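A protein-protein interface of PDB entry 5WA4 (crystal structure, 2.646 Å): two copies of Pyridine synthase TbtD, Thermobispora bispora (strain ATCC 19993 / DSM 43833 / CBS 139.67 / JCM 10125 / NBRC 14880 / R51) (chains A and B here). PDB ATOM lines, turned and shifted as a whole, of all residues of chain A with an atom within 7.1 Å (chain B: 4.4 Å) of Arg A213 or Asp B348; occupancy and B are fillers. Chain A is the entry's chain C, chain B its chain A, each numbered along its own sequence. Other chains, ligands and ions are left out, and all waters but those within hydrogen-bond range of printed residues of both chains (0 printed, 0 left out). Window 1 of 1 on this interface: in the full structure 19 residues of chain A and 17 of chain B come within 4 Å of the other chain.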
ATOM      1  N   ARG A 192       9.678 -20.825 -19.982  1.00  0.00           N
ATOM      2  CA  ARG A 192       8.325 -21.075 -20.458  1.00  0.00           C
ATOM      3  C   ARG A 192       7.769 -22.382 -19.893  1.00  0.00           C
ATOM      4  O   ARG A 192       6.591 -22.462 -19.507  1.00  0.00           O
ATOM      5  CB  ARG A 192       8.267 -21.101 -21.991  1.00  0.00           C
ATOM      6  CG  ARG A 192       6.819 -21.105 -22.523  1.00  0.00           C
ATOM      7  CD  ARG A 192       6.771 -21.105 -24.026  1.00  0.00           C
ATOM      8  NE  ARG A 192       7.533 -20.009 -24.626  1.00  0.00           N
ATOM      9  CZ  ARG A 192       7.115 -18.747 -24.662  1.00  0.00           C
ATOM     10  NH1 ARG A 192       5.959 -18.405 -24.110  1.00  0.00           N
ATOM     11  NH2 ARG A 192       7.857 -17.822 -25.254  1.00  0.00           N
ATOM     12  N   ARG A 207      -7.616 -18.251 -21.014  1.00  0.00           N
ATOM     13  CA  ARG A 207      -7.870 -16.828 -20.722  1.00  0.00           C
ATOM     14  C   ARG A 207      -6.684 -16.165 -19.978  1.00  0.00           C
ATOM     15  O   ARG A 207      -6.387 -14.987 -20.215  1.00  0.00           O
ATOM     16  CB  ARG A 207      -9.155 -16.628 -19.915  1.00  0.00           C
ATOM     17  CG  ARG A 207      -9.396 -15.163 -19.545  1.00  0.00           C
ATOM     18  CD  ARG A 207     -10.412 -14.523 -20.485  1.00  0.00           C
ATOM     19  NE  ARG A 207      -9.992 -13.205 -20.978  1.00  0.00           N
ATOM     20  CZ  ARG A 207     -10.540 -12.586 -22.027  1.00  0.00           C
ATOM     21  NH1 ARG A 207     -11.540 -13.164 -22.691  1.00  0.00           N
ATOM     22  NH2 ARG A 207     -10.094 -11.389 -22.408  1.00  0.00           N
ATOM     23  N   LEU A 208      -5.994 -16.909 -19.109  1.00  0.00           N
ATOM     24  CA  LEU A 208      -4.745 -16.399 -18.557  1.00  0.00           C
ATOM     25  C   LEU A 208      -3.720 -16.056 -19.634  1.00  0.00           C
ATOM     26  O   LEU A 208      -3.126 -14.972 -19.584  1.00  0.00           O
ATOM     27  CB  LEU A 208      -4.123 -17.387 -17.565  1.00  0.00           C
ATOM     28  CG  LEU A 208      -4.667 -17.380 -16.129  1.00  0.00           C
ATOM     29  CD1 LEU A 208      -3.873 -18.328 -15.261  1.00  0.00           C
ATOM     30  CD2 LEU A 208      -4.685 -15.973 -15.539  1.00  0.00           C
ATOM     31  N   ARG A 209      -3.497 -16.961 -20.592  1.00  0.00           N
ATOM     32  CA  ARG A 209      -2.516 -16.713 -21.653  1.00  0.00           C
ATOM     33  C   ARG A 209      -2.854 -15.471 -22.464  1.00  0.00           C
ATOM     34  O   ARG A 209      -1.954 -14.760 -22.893  1.00  0.00           O
ATOM     35  CB  ARG A 209      -2.418 -17.895 -22.599  1.00  0.00           C
ATOM     36  CG  ARG A 209      -2.058 -19.201 -21.967  1.00  0.00           C
ATOM     37  CD  ARG A 209      -2.674 -20.324 -22.777  1.00  0.00           C
ATOM     38  NE  ARG A 209      -2.510 -21.641 -22.170  1.00  0.00           N
ATOM     39  CZ  ARG A 209      -1.334 -22.254 -22.071  1.00  0.00           C
ATOM     40  NH1 ARG A 209      -0.219 -21.625 -22.524  1.00  0.00           N
ATOM     41  NH2 ARG A 209      -1.282 -23.472 -21.499  1.00  0.00           N
ATOM     42  N   GLU A 210      -4.136 -15.183 -22.679  1.00  0.00           N
ATOM     43  CA  GLU A 210      -4.440 -13.973 -23.426  1.00  0.00           C
ATOM     44  C   GLU A 210      -4.093 -12.716 -22.649  1.00  0.00           C
ATOM     45  O   GLU A 210      -3.437 -11.831 -23.209  1.00  0.00           O
ATOM     46  CB  GLU A 210      -5.894 -13.931 -23.887  1.00  0.00           C
ATOM     47  CG  GLU A 210      -5.950 -13.511 -25.366  1.00  0.00           C
ATOM     48  CD  GLU A 210      -6.988 -14.259 -26.190  1.00  0.00           C
ATOM     49  OE1 GLU A 210      -8.193 -14.145 -25.868  1.00  0.00           O
ATOM     50  OE2 GLU A 210      -6.582 -14.977 -27.145  1.00  0.00           O
ATOM     51  N   LEU A 211      -4.500 -12.649 -21.376  1.00  0.00           N
ATOM     52  CA  LEU A 211      -4.072 -11.578 -20.451  1.00  0.00           C
ATOM     53  C   LEU A 211      -2.568 -11.379 -20.493  1.00  0.00           C
ATOM     54  O   LEU A 211      -2.084 -10.269 -20.723  1.00  0.00           O
ATOM     55  CB  LEU A 211      -4.501 -11.890 -19.017  1.00  0.00           C
ATOM     56  CG  LEU A 211      -6.008 -11.753 -18.763  1.00  0.00           C
ATOM     57  CD1 LEU A 211      -6.415 -12.261 -17.390  1.00  0.00           C
ATOM     58  CD2 LEU A 211      -6.450 -10.310 -18.949  1.00  0.00           C
ATOM     59  N   TRP A 212      -1.825 -12.465 -20.323  1.00  0.00           N
ATOM     60  CA  TRP A 212      -0.391 -12.317 -20.209  1.00  0.00           C
ATOM     61  C   TRP A 212       0.227 -11.929 -21.553  1.00  0.00           C
ATOM     62  O   TRP A 212       1.233 -11.202 -21.571  1.00  0.00           O
ATOM     63  CB  TRP A 212       0.251 -13.595 -19.618  1.00  0.00           C
ATOM     64  CG  TRP A 212      -0.234 -13.894 -18.189  1.00  0.00           C
ATOM     65  CD1 TRP A 212      -1.147 -13.166 -17.470  1.00  0.00           C
ATOM     66  CD2 TRP A 212       0.129 -14.996 -17.355  1.00  0.00           C
ATOM     67  NE1 TRP A 212      -1.374 -13.745 -16.262  1.00  0.00           N
ATOM     68  CE2 TRP A 212      -0.593 -14.869 -16.148  1.00  0.00           C
ATOM     69  CE3 TRP A 212       1.002 -16.083 -17.501  1.00  0.00           C
ATOM     70  CZ2 TRP A 212      -0.477 -15.769 -15.089  1.00  0.00           C
ATOM     71  CZ3 TRP A 212       1.123 -16.991 -16.445  1.00  0.00           C
ATOM     72  CH2 TRP A 212       0.387 -16.823 -15.252  1.00  0.00           C
ATOM     73  N   ARG A 213      -0.362 -12.361 -22.678  1.00  0.00           N
ATOM     74  CA  ARG A 213       0.251 -11.992 -23.954  1.00  0.00           C
ATOM     75  C   ARG A 213      -0.155 -10.590 -24.407  1.00  0.00           C
ATOM     76  O   ARG A 213       0.687  -9.837 -24.917  1.00  0.00           O
ATOM     77  CB  ARG A 213      -0.035 -13.004 -25.072  1.00  0.00           C
ATOM     78  CG  ARG A 213       0.921 -12.723 -26.244  1.00  0.00           C
ATOM     79  CD  ARG A 213       1.584 -13.977 -26.734  1.00  0.00           C
ATOM     80  NE  ARG A 213       2.927 -13.776 -27.321  1.00  0.00           N
ATOM     81  CZ  ARG A 213       3.256 -13.061 -28.400  1.00  0.00           C
ATOM     82  NH1 ARG A 213       2.339 -12.460 -29.163  1.00  0.00           N
ATOM     83  NH2 ARG A 213       4.535 -13.007 -28.747  1.00  0.00           N
ATOM     84  N   ASP A 214      -1.416 -10.224 -24.216  1.00  0.00           N
ATOM     85  CA  ASP A 214      -1.768  -8.825 -24.399  1.00  0.00           C
ATOM     86  C   ASP A 214      -0.827  -7.936 -23.587  1.00  0.00           C
ATOM     87  O   ASP A 214      -0.358  -6.918 -24.096  1.00  0.00           O
ATOM     88  CB  ASP A 214      -3.199  -8.529 -23.970  1.00  0.00           C
ATOM     89  CG  ASP A 214      -4.216  -9.164 -24.844  1.00  0.00           C
ATOM     90  OD1 ASP A 214      -3.877  -9.621 -25.955  1.00  0.00           O
ATOM     91  OD2 ASP A 214      -5.377  -9.183 -24.418  1.00  0.00           O
ATOM     92  N   HIS A 215      -0.547  -8.317 -22.335  1.00  0.00           N
ATOM     93  CA  HIS A 215       0.266  -7.458 -21.495  1.00  0.00           C
ATOM     94  C   HIS A 215       1.689  -7.359 -22.039  1.00  0.00           C
ATOM     95  O   HIS A 215       2.293  -6.279 -22.024  1.00  0.00           O
ATOM     96  CB  HIS A 215       0.294  -7.925 -20.029  1.00  0.00           C
ATOM     97  CG  HIS A 215       1.171  -7.071 -19.160  1.00  0.00           C
ATOM     98  ND1 HIS A 215       0.707  -5.950 -18.502  1.00  0.00           N
ATOM     99  CD2 HIS A 215       2.502  -7.135 -18.897  1.00  0.00           C
ATOM    100  CE1 HIS A 215       1.705  -5.377 -17.851  1.00  0.00           C
ATOM    101  NE2 HIS A 215       2.806  -6.076 -18.076  1.00  0.00           N
ATOM    102  N   TYR A 216       2.224  -8.480 -22.515  1.00  0.00           N
ATOM    103  CA  TYR A 216       3.539  -8.451 -23.137  1.00  0.00           C
ATOM    104  C   TYR A 216       3.517  -7.566 -24.385  1.00  0.00           C
ATOM    105  O   TYR A 216       4.508  -6.915 -24.715  1.00  0.00           O
ATOM    106  CB  TYR A 216       4.013  -9.854 -23.502  1.00  0.00           C
ATOM    107  CG  TYR A 216       5.319  -9.831 -24.246  1.00  0.00           C
ATOM    108  CD1 TYR A 216       6.507  -9.768 -23.563  1.00  0.00           C
ATOM    109  CD2 TYR A 216       5.362  -9.822 -25.639  1.00  0.00           C
ATOM    110  CE1 TYR A 216       7.713  -9.733 -24.219  1.00  0.00           C
ATOM    111  CE2 TYR A 216       6.578  -9.783 -26.317  1.00  0.00           C
ATOM    112  CZ  TYR A 216       7.750  -9.741 -25.588  1.00  0.00           C
ATOM    113  OH  TYR A 216       8.979  -9.700 -26.199  1.00  0.00           O
ATOM    114  N   ALA A 217       2.386  -7.548 -25.081  1.00  0.00           N
ATOM    115  CA  ALA A 217       2.315  -6.825 -26.342  1.00  0.00           C
ATOM    116  C   ALA A 217       2.297  -5.327 -26.095  1.00  0.00           C
ATOM    117  O   ALA A 217       2.975  -4.563 -26.792  1.00  0.00           O
ATOM    118  CB  ALA A 217       1.083  -7.258 -27.150  1.00  0.00           C
ATOM    119  N   ARG A 218       1.516  -4.924 -25.096  1.00  0.00           N
ATOM    120  CA  ARG A 218       1.434  -3.531 -24.676  1.00  0.00           C
ATOM    121  C   ARG A 218       2.793  -2.956 -24.324  1.00  0.00           C
ATOM    122  O   ARG A 218       2.998  -1.752 -24.395  1.00  0.00           O
ATOM    123  CB  ARG A 218       0.542  -3.381 -23.448  1.00  0.00           C
ATOM    124  CG  ARG A 218      -0.914  -3.604 -23.632  1.00  0.00           C
ATOM    125  CD  ARG A 218      -1.621  -3.227 -22.344  1.00  0.00           C
ATOM    126  NE  ARG A 218      -2.626  -4.216 -21.998  1.00  0.00           N
ATOM    127  CZ  ARG A 218      -2.488  -5.096 -21.017  1.00  0.00           C
ATOM    128  NH1 ARG A 218      -1.391  -5.075 -20.270  1.00  0.00           N
ATOM    129  NH2 ARG A 218      -3.456  -5.980 -20.771  1.00  0.00           N
ATOM    130  N   ASN A 219       3.712  -3.824 -23.918  1.00  0.00           N
ATOM    131  CA  ASN A 219       4.916  -3.390 -23.220  1.00  0.00           C
ATOM    132  C   ASN A 219       6.134  -4.101 -23.726  1.00  0.00           C
ATOM    133  O   ASN A 219       7.065  -4.380 -22.969  1.00  0.00           O
ATOM    134  CB  ASN A 219       4.759  -3.622 -21.717  1.00  0.00           C
ATOM    135  CG  ASN A 219       3.652  -2.780 -21.136  1.00  0.00           C
ATOM    136  OD1 ASN A 219       3.753  -1.550 -21.130  1.00  0.00           O
ATOM    137  ND2 ASN A 219       2.578  -3.419 -20.677  1.00  0.00           N
ATOM    138  N   ARG A 220       6.125  -4.382 -25.020  1.00  0.00           N
ATOM    139  CA  ARG A 220       7.129  -5.250 -25.604  1.00  0.00           C
ATOM    140  C   ARG A 220       8.525  -4.685 -25.423  1.00  0.00           C
ATOM    141  O   ARG A 220       9.423  -5.415 -25.034  1.00  0.00           O
ATOM    142  CB  ARG A 220       6.835  -5.486 -27.083  1.00  0.00           C
ATOM    143  CG  ARG A 220       7.649  -6.617 -27.744  1.00  0.00           C
ATOM    144  CD  ARG A 220       7.208  -6.837 -29.196  1.00  0.00           C
ATOM    145  NE  ARG A 220       5.912  -6.206 -29.466  1.00  0.00           N
ATOM    146  CZ  ARG A 220       5.766  -5.001 -30.016  1.00  0.00           C
ATOM    147  NH1 ARG A 220       6.847  -4.302 -30.354  1.00  0.00           N
ATOM    148  NH2 ARG A 220       4.552  -4.490 -30.218  1.00  0.00           N
ATOM    149  N   LEU A 337       3.687 -15.770 -13.871  1.00  0.00           N
ATOM    150  CA  LEU A 337       3.552 -14.591 -14.714  1.00  0.00           C
ATOM    151  C   LEU A 337       4.913 -14.093 -15.170  1.00  0.00           C
ATOM    152  O   LEU A 337       5.199 -14.057 -16.368  1.00  0.00           O
ATOM    153  CB  LEU A 337       2.784 -13.495 -13.973  1.00  0.00           C
ATOM    154  CG  LEU A 337       2.616 -12.156 -14.689  1.00  0.00           C
ATOM    155  CD1 LEU A 337       2.114 -12.331 -16.108  1.00  0.00           C
ATOM    156  CD2 LEU A 337       1.633 -11.299 -13.913  1.00  0.00           C
ATOM    157  N   HIS A 340       6.585 -16.309 -17.544  1.00  0.00           N
ATOM    158  CA  HIS A 340       5.976 -16.269 -18.875  1.00  0.00           C
ATOM    159  C   HIS A 340       6.523 -15.063 -19.631  1.00  0.00           C
ATOM    160  O   HIS A 340       7.140 -15.218 -20.699  1.00  0.00           O
ATOM    161  CB  HIS A 340       4.435 -16.214 -18.803  1.00  0.00           C
ATOM    162  CG  HIS A 340       3.758 -16.469 -20.113  1.00  0.00           C
ATOM    163  ND1 HIS A 340       3.352 -15.450 -20.960  1.00  0.00           N
ATOM    164  CD2 HIS A 340       3.441 -17.628 -20.737  1.00  0.00           C
ATOM    165  CE1 HIS A 340       2.802 -15.978 -22.037  1.00  0.00           C
ATOM    166  NE2 HIS A 340       2.845 -17.294 -21.931  1.00  0.00           N
ATOM    167  N   LEU A 341       6.331 -13.872 -19.059  1.00  0.00           N
ATOM    168  CA  LEU A 341       6.846 -12.651 -19.678  1.00  0.00           C
ATOM    169  C   LEU A 341       8.340 -12.714 -19.979  1.00  0.00           C
ATOM    170  O   LEU A 341       8.772 -12.194 -20.992  1.00  0.00           O
ATOM    171  CB  LEU A 341       6.565 -11.450 -18.799  1.00  0.00           C
ATOM    172  CG  LEU A 341       5.099 -11.221 -18.503  1.00  0.00           C
ATOM    173  CD1 LEU A 341       5.038 -10.411 -17.224  1.00  0.00           C
ATOM    174  CD2 LEU A 341       4.466 -10.453 -19.636  1.00  0.00           C
ATOM    175  N   ASP A 344       8.597 -14.948 -23.178  1.00  0.00           N
ATOM    176  CA  ASP A 344       8.090 -14.241 -24.346  1.00  0.00           C
ATOM    177  C   ASP A 344       9.090 -13.213 -24.851  1.00  0.00           C
ATOM    178  O   ASP A 344       9.252 -13.023 -26.056  1.00  0.00           O
ATOM    179  CB  ASP A 344       6.749 -13.574 -24.034  1.00  0.00           C
ATOM    180  CG  ASP A 344       5.572 -14.437 -24.465  1.00  0.00           C
ATOM    181  OD1 ASP A 344       5.811 -15.625 -24.813  1.00  0.00           O
ATOM    182  OD2 ASP A 344       4.422 -13.936 -24.466  1.00  0.00           O
ATOM    183  N   ALA A 347      11.779 -14.786 -26.683  1.00  0.00           N
ATOM    184  CA  ALA A 347      11.320 -15.040 -28.045  1.00  0.00           C
ATOM    185  C   ALA A 347      11.661 -13.874 -28.984  1.00  0.00           C
ATOM    186  O   ALA A 347      12.304 -14.059 -30.013  1.00  0.00           O
ATOM    187  CB  ALA A 347       9.820 -15.310 -28.051  1.00  0.00           C
ATOM    188  N   ASP A 348      11.245 -12.666 -28.625  1.00  0.00           N
ATOM    189  CA  ASP A 348      11.550 -11.506 -29.447  1.00  0.00           C
ATOM    190  C   ASP A 348      13.037 -11.114 -29.504  1.00  0.00           C
ATOM    191  O   ASP A 348      13.408 -10.218 -30.255  1.00  0.00           O
ATOM    192  CB  ASP A 348      10.750 -10.304 -28.969  1.00  0.00           C
ATOM    193  CG  ASP A 348       9.314 -10.369 -29.387  1.00  0.00           C
ATOM    194  OD1 ASP A 348       8.520 -11.025 -28.677  1.00  0.00           O
ATOM    195  OD2 ASP A 348       8.972  -9.769 -30.430  1.00  0.00           O
ATOM    196  N   ARG B 213       5.928 -19.220 -31.469  1.00  0.00           N
ATOM    197  CA  ARG B 213       6.093 -17.838 -31.057  1.00  0.00           C
ATOM    198  C   ARG B 213       7.388 -17.217 -31.606  1.00  0.00           C
ATOM    199  O   ARG B 213       7.428 -16.010 -31.897  1.00  0.00           O
ATOM    200  CB  ARG B 213       6.062 -17.699 -29.538  1.00  0.00           C
ATOM    201  CG  ARG B 213       5.980 -16.236 -29.130  1.00  0.00           C
ATOM    202  CD  ARG B 213       5.195 -16.063 -27.877  1.00  0.00           C
ATOM    203  NE  ARG B 213       3.846 -16.616 -27.964  1.00  0.00           N
ATOM    204  CZ  ARG B 213       3.028 -16.725 -26.921  1.00  0.00           C
ATOM    205  NH1 ARG B 213       3.410 -16.303 -25.732  1.00  0.00           N
ATOM    206  NH2 ARG B 213       1.820 -17.225 -27.078  1.00  0.00           N
ATOM    207  N   TYR B 216       6.183 -16.249 -35.094  1.00  0.00           N
ATOM    208  CA  TYR B 216       5.345 -15.063 -35.092  1.00  0.00           C
ATOM    209  C   TYR B 216       6.199 -13.836 -34.870  1.00  0.00           C
ATOM    210  O   TYR B 216       6.013 -12.824 -35.534  1.00  0.00           O
ATOM    211  CB  TYR B 216       4.274 -15.143 -34.021  1.00  0.00           C
ATOM    212  CG  TYR B 216       3.456 -13.885 -33.928  1.00  0.00           C
ATOM    213  CD1 TYR B 216       3.880 -12.817 -33.164  1.00  0.00           C
ATOM    214  CD2 TYR B 216       2.257 -13.772 -34.595  1.00  0.00           C
ATOM    215  CE1 TYR B 216       3.142 -11.662 -33.081  1.00  0.00           C
ATOM    216  CE2 TYR B 216       1.499 -12.625 -34.518  1.00  0.00           C
ATOM    217  CZ  TYR B 216       1.947 -11.569 -33.756  1.00  0.00           C
ATOM    218  OH  TYR B 216       1.209 -10.412 -33.666  1.00  0.00           O
ATOM    219  N   ARG B 220       6.265 -10.436 -37.396  1.00  0.00           N
ATOM    220  CA  ARG B 220       5.040  -9.950 -36.741  1.00  0.00           C
ATOM    221  C   ARG B 220       4.191  -8.992 -37.574  1.00  0.00           C
ATOM    222  O   ARG B 220       2.955  -9.085 -37.576  1.00  0.00           O
ATOM    223  CB  ARG B 220       5.382  -9.279 -35.405  1.00  0.00           C
ATOM    224  CG  ARG B 220       4.197  -8.620 -34.688  1.00  0.00           C
ATOM    225  CD  ARG B 220       4.533  -8.236 -33.228  1.00  0.00           C
ATOM    226  NE  ARG B 220       5.780  -7.478 -33.129  1.00  0.00           N
ATOM    227  CZ  ARG B 220       6.970  -8.015 -32.844  1.00  0.00           C
ATOM    228  NH1 ARG B 220       7.083  -9.320 -32.613  1.00  0.00           N
ATOM    229  NH2 ARG B 220       8.053  -7.244 -32.788  1.00  0.00           N
ATOM    230  N   THR B 224      -0.071  -8.997 -38.717  1.00  0.00           N
ATOM    231  CA  THR B 224      -1.040  -8.033 -38.200  1.00  0.00           C
ATOM    232  C   THR B 224      -1.654  -7.200 -39.317  1.00  0.00           C
ATOM    233  O   THR B 224      -2.873  -7.001 -39.365  1.00  0.00           O
ATOM    234  CB  THR B 224      -0.406  -7.110 -37.148  1.00  0.00           C
ATOM    235  OG1 THR B 224       0.989  -6.947 -37.442  1.00  0.00           O
ATOM    236  CG2 THR B 224      -0.545  -7.724 -35.778  1.00  0.00           C
ATOM    237  N   ASP B 344      -2.280 -14.793 -31.796  1.00  0.00           N
ATOM    238  CA  ASP B 344      -1.144 -13.950 -31.471  1.00  0.00           C
ATOM    239  C   ASP B 344      -1.272 -12.615 -32.170  1.00  0.00           C
ATOM    240  O   ASP B 344      -1.192 -11.582 -31.529  1.00  0.00           O
ATOM    241  CB  ASP B 344       0.169 -14.625 -31.836  1.00  0.00           C
ATOM    242  CG  ASP B 344       0.747 -15.439 -30.684  1.00  0.00           C
ATOM    243  OD1 ASP B 344       0.013 -15.693 -29.701  1.00  0.00           O
ATOM    244  OD2 ASP B 344       1.943 -15.822 -30.761  1.00  0.00           O
ATOM    245  N   ALA B 345      -1.516 -12.636 -33.473  1.00  0.00           N
ATOM    246  CA  ALA B 345      -1.673 -11.407 -34.240  1.00  0.00           C
ATOM    247  C   ALA B 345      -2.767 -10.504 -33.672  1.00  0.00           C
ATOM    248  O   ALA B 345      -2.604  -9.284 -33.622  1.00  0.00           O
ATOM    249  CB  ALA B 345      -1.957 -11.731 -35.674  1.00  0.00           C
ATOM    250  N   ALA B 346      -3.866 -11.105 -33.228  1.00  0.00           N
ATOM    251  CA  ALA B 346      -4.950 -10.339 -32.634  1.00  0.00           C
ATOM    252  C   ALA B 346      -4.519  -9.606 -31.344  1.00  0.00           C
ATOM    253  O   ALA B 346      -5.015  -8.511 -31.048  1.00  0.00           O
ATOM    254  CB  ALA B 346      -6.117 -11.241 -32.354  1.00  0.00           C
ATOM    255  N   ALA B 347      -3.595 -10.204 -30.588  1.00  0.00           N
ATOM    256  CA  ALA B 347      -3.121  -9.612 -29.342  1.00  0.00           C
ATOM    257  C   ALA B 347      -2.463  -8.255 -29.590  1.00  0.00           C
ATOM    258  O   ALA B 347      -2.808  -7.270 -28.937  1.00  0.00           O
ATOM    259  CB  ALA B 347      -2.155 -10.551 -28.640  1.00  0.00           C
ATOM    260  N   ASP B 348      -1.528  -8.198 -30.535  1.00  0.00           N
ATOM    261  CA  ASP B 348      -0.894  -6.934 -30.927  1.00  0.00           C
ATOM    262  C   ASP B 348      -1.866  -5.957 -31.617  1.00  0.00           C
ATOM    263  O   ASP B 348      -1.491  -4.831 -31.947  1.00  0.00           O
ATOM    264  CB  ASP B 348       0.293  -7.196 -31.856  1.00  0.00           C
ATOM    265  CG  ASP B 348       1.427  -7.915 -31.170  1.00  0.00           C
ATOM    266  OD1 ASP B 348       1.271  -9.104 -30.829  1.00  0.00           O
ATOM    267  OD2 ASP B 348       2.505  -7.310 -31.012  1.00  0.00           O
ATOM    268  N   VAL B 349      -3.104  -6.385 -31.853  1.00  0.00           N
ATOM    269  CA  VAL B 349      -4.072  -5.519 -32.516  1.00  0.00           C
ATOM    270  C   VAL B 349      -5.179  -5.113 -31.571  1.00  0.00           C
ATOM    271  O   VAL B 349      -5.444  -3.935 -31.386  1.00  0.00           O
ATOM    272  CB  VAL B 349      -4.704  -6.188 -33.770  1.00  0.00           C
ATOM    273  CG1 VAL B 349      -5.886  -5.352 -34.298  1.00  0.00           C
ATOM    274  CG2 VAL B 349      -3.660  -6.363 -34.868  1.00  0.00           C
ATOM    275  N   TYR B 350      -5.839  -6.090 -30.977  1.00  0.00           N
ATOM    276  CA  TYR B 350      -6.975  -5.790 -30.121  1.00  0.00           C
ATOM    277  C   TYR B 350      -6.596  -5.822 -28.641  1.00  0.00           C
ATOM    278  O   TYR B 350      -7.462  -5.754 -27.770  1.00  0.00           O
ATOM    279  CB  TYR B 350      -8.120  -6.769 -30.403  1.00  0.00           C
ATOM    280  CG  TYR B 350      -8.782  -6.520 -31.736  1.00  0.00           C
ATOM    281  CD1 TYR B 350      -8.323  -7.150 -32.881  1.00  0.00           C
ATOM    282  CD2 TYR B 350      -9.861  -5.643 -31.851  1.00  0.00           C
ATOM    283  CE1 TYR B 350      -8.911  -6.920 -34.100  1.00  0.00           C
ATOM    284  CE2 TYR B 350     -10.459  -5.405 -33.063  1.00  0.00           C
ATOM    285  CZ  TYR B 350      -9.980  -6.050 -34.193  1.00  0.00           C
ATOM    286  OH  TYR B 350     -10.556  -5.831 -35.429  1.00  0.00           O
ATOM    287  N   ILE B 352      -3.908  -3.804 -27.354  1.00  0.00           N
ATOM    288  CA  ILE B 352      -3.197  -2.605 -26.928  1.00  0.00           C
ATOM    289  C   ILE B 352      -4.088  -1.358 -26.935  1.00  0.00           C
ATOM    290  O   ILE B 352      -3.589  -0.230 -26.835  1.00  0.00           O
ATOM    291  CB  ILE B 352      -1.946  -2.358 -27.790  1.00  0.00           C
ATOM    292  CG1 ILE B 352      -2.303  -2.118 -29.252  1.00  0.00           C
ATOM    293  CG2 ILE B 352      -0.997  -3.546 -27.700  1.00  0.00           C
ATOM    294  CD1 ILE B 352      -1.059  -1.961 -30.128  1.00  0.00           C
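Arg B213 touches Arg A192.
Asp A214 touches Ala B347 (OD1 to CB, 3.3 Å).
CG2 of Ile B352 touches N of Arg A218 (3.9 Å).
Arg A220 touches Arg B220.
His A340 touches Arg B213 (CE1 to NH1, 3.8 Å).
Printed residues of chain A that touch a printed residue of chain B: Arg A192, Arg A213, Asp A214, Arg A218, Arg A220, His A340, Asp A344 and Asp A348.
Printed residues of chain B that touch a printed residue of chain A: Arg B213, Arg B220, Asp B344, Ala B347, Asp B348 and Ile B352.
Among the printed residues, 11 pairs touch across the chains.
Among the printed residues, Asp or Glu carboxylates within 4 Å of a Lys or Arg side-chain nitrogen of the other chain: Arg A213 with Asp B344 (3.7 Å), Arg A213 with Asp B348 (3.9 Å), Arg A220 with Asp B348 (3.6 Å), Asp A344 with Arg B213 (2.7 Å) and Asp A348 with Arg B220 (2.9 Å).
Of the printed residues of chain B, Arg A220 touches Arg B220 (3.7 Å) and Asp B348 (3.6 Å).
Printed residues of chain B within 4 Å of His A340: Arg B213 (3.8 Å).
Printed residues of chain A within 4 Å of Arg B213: Arg A192, Arg A213, His A340 and Asp A344.
Thr B224 touches none of the printed residues of chain A.
Ala B346 touches none of the printed residues of chain A.
Of chain A, only Arg A213 (3.9 Å) and Arg A220 (3.6 Å) come within 4 Å of Asp B348.
The nearest residue of chain B that does not touch Arg A213 is Tyr B216 (4.1 Å).
OD2 of Asp A344 is in salt-bridge range of NE of Arg A213 (3.2 Å).
OD2 of Asp B348 is in salt-bridge range of NE of Arg B220 (3.9 Å).
The side-chain hydroxyl (OH) of Tyr B216 is in hydrogen-bond range of the side-chain carboxylate (OD1) of Asp B348, at 3.1 Å.
The backbone carbonyl oxygen (O) of Arg B220 lies within hydrogen-bond range of the side-chain hydroxyl (OG1) of Thr B224.
The side-chain hydroxyl (OH) of Tyr A216 sits at hydrogen-bond distance from the side-chain carboxylate (OD1) of Asp A348 (2.8 Å).
The side-chain carboxylate of Asp B344 lies within salt-bridge range of the guanidinium group of Arg B213.
The guanidinium group of Arg A213 sits close to the guanidinium group of Arg B213, 3.0 Å away.
The side-chain carboxylate (OD1) of Asp B348 is in salt-bridge range of the guanidinium group (NH1) of Arg A213, 3.9 Å away.
The side-chain carboxylate (OD2) of Asp B344 is in salt-bridge range of the guanidinium group (NH1) of Arg A213, 3.7 Å away.
The side-chain carboxylate (OD1) of Asp A344 lies within salt-bridge range of the guanidinium group (NH1) of Arg B213 (2.7 Å).
The guanidinium group of Arg B220 is in salt-bridge range of the side-chain carboxylate of Asp A348 (2.9 Å).
The side-chain carboxylate of Asp B348 is in salt-bridge range of the guanidinium group of Arg A220 (3.6 Å).
Arg A213 touches Asp B344, and with the chains exchanged Asp A344 touches Arg B213.
Arg A213 touches Asp B348, but with the chains exchanged Asp A348 does not touch Arg B213 (5.8 Å).
Arg A220 touches its own counterpart, Arg B220.
Arg A220 touches Asp B348, and with the chains exchanged Asp A348 touches Arg B220.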
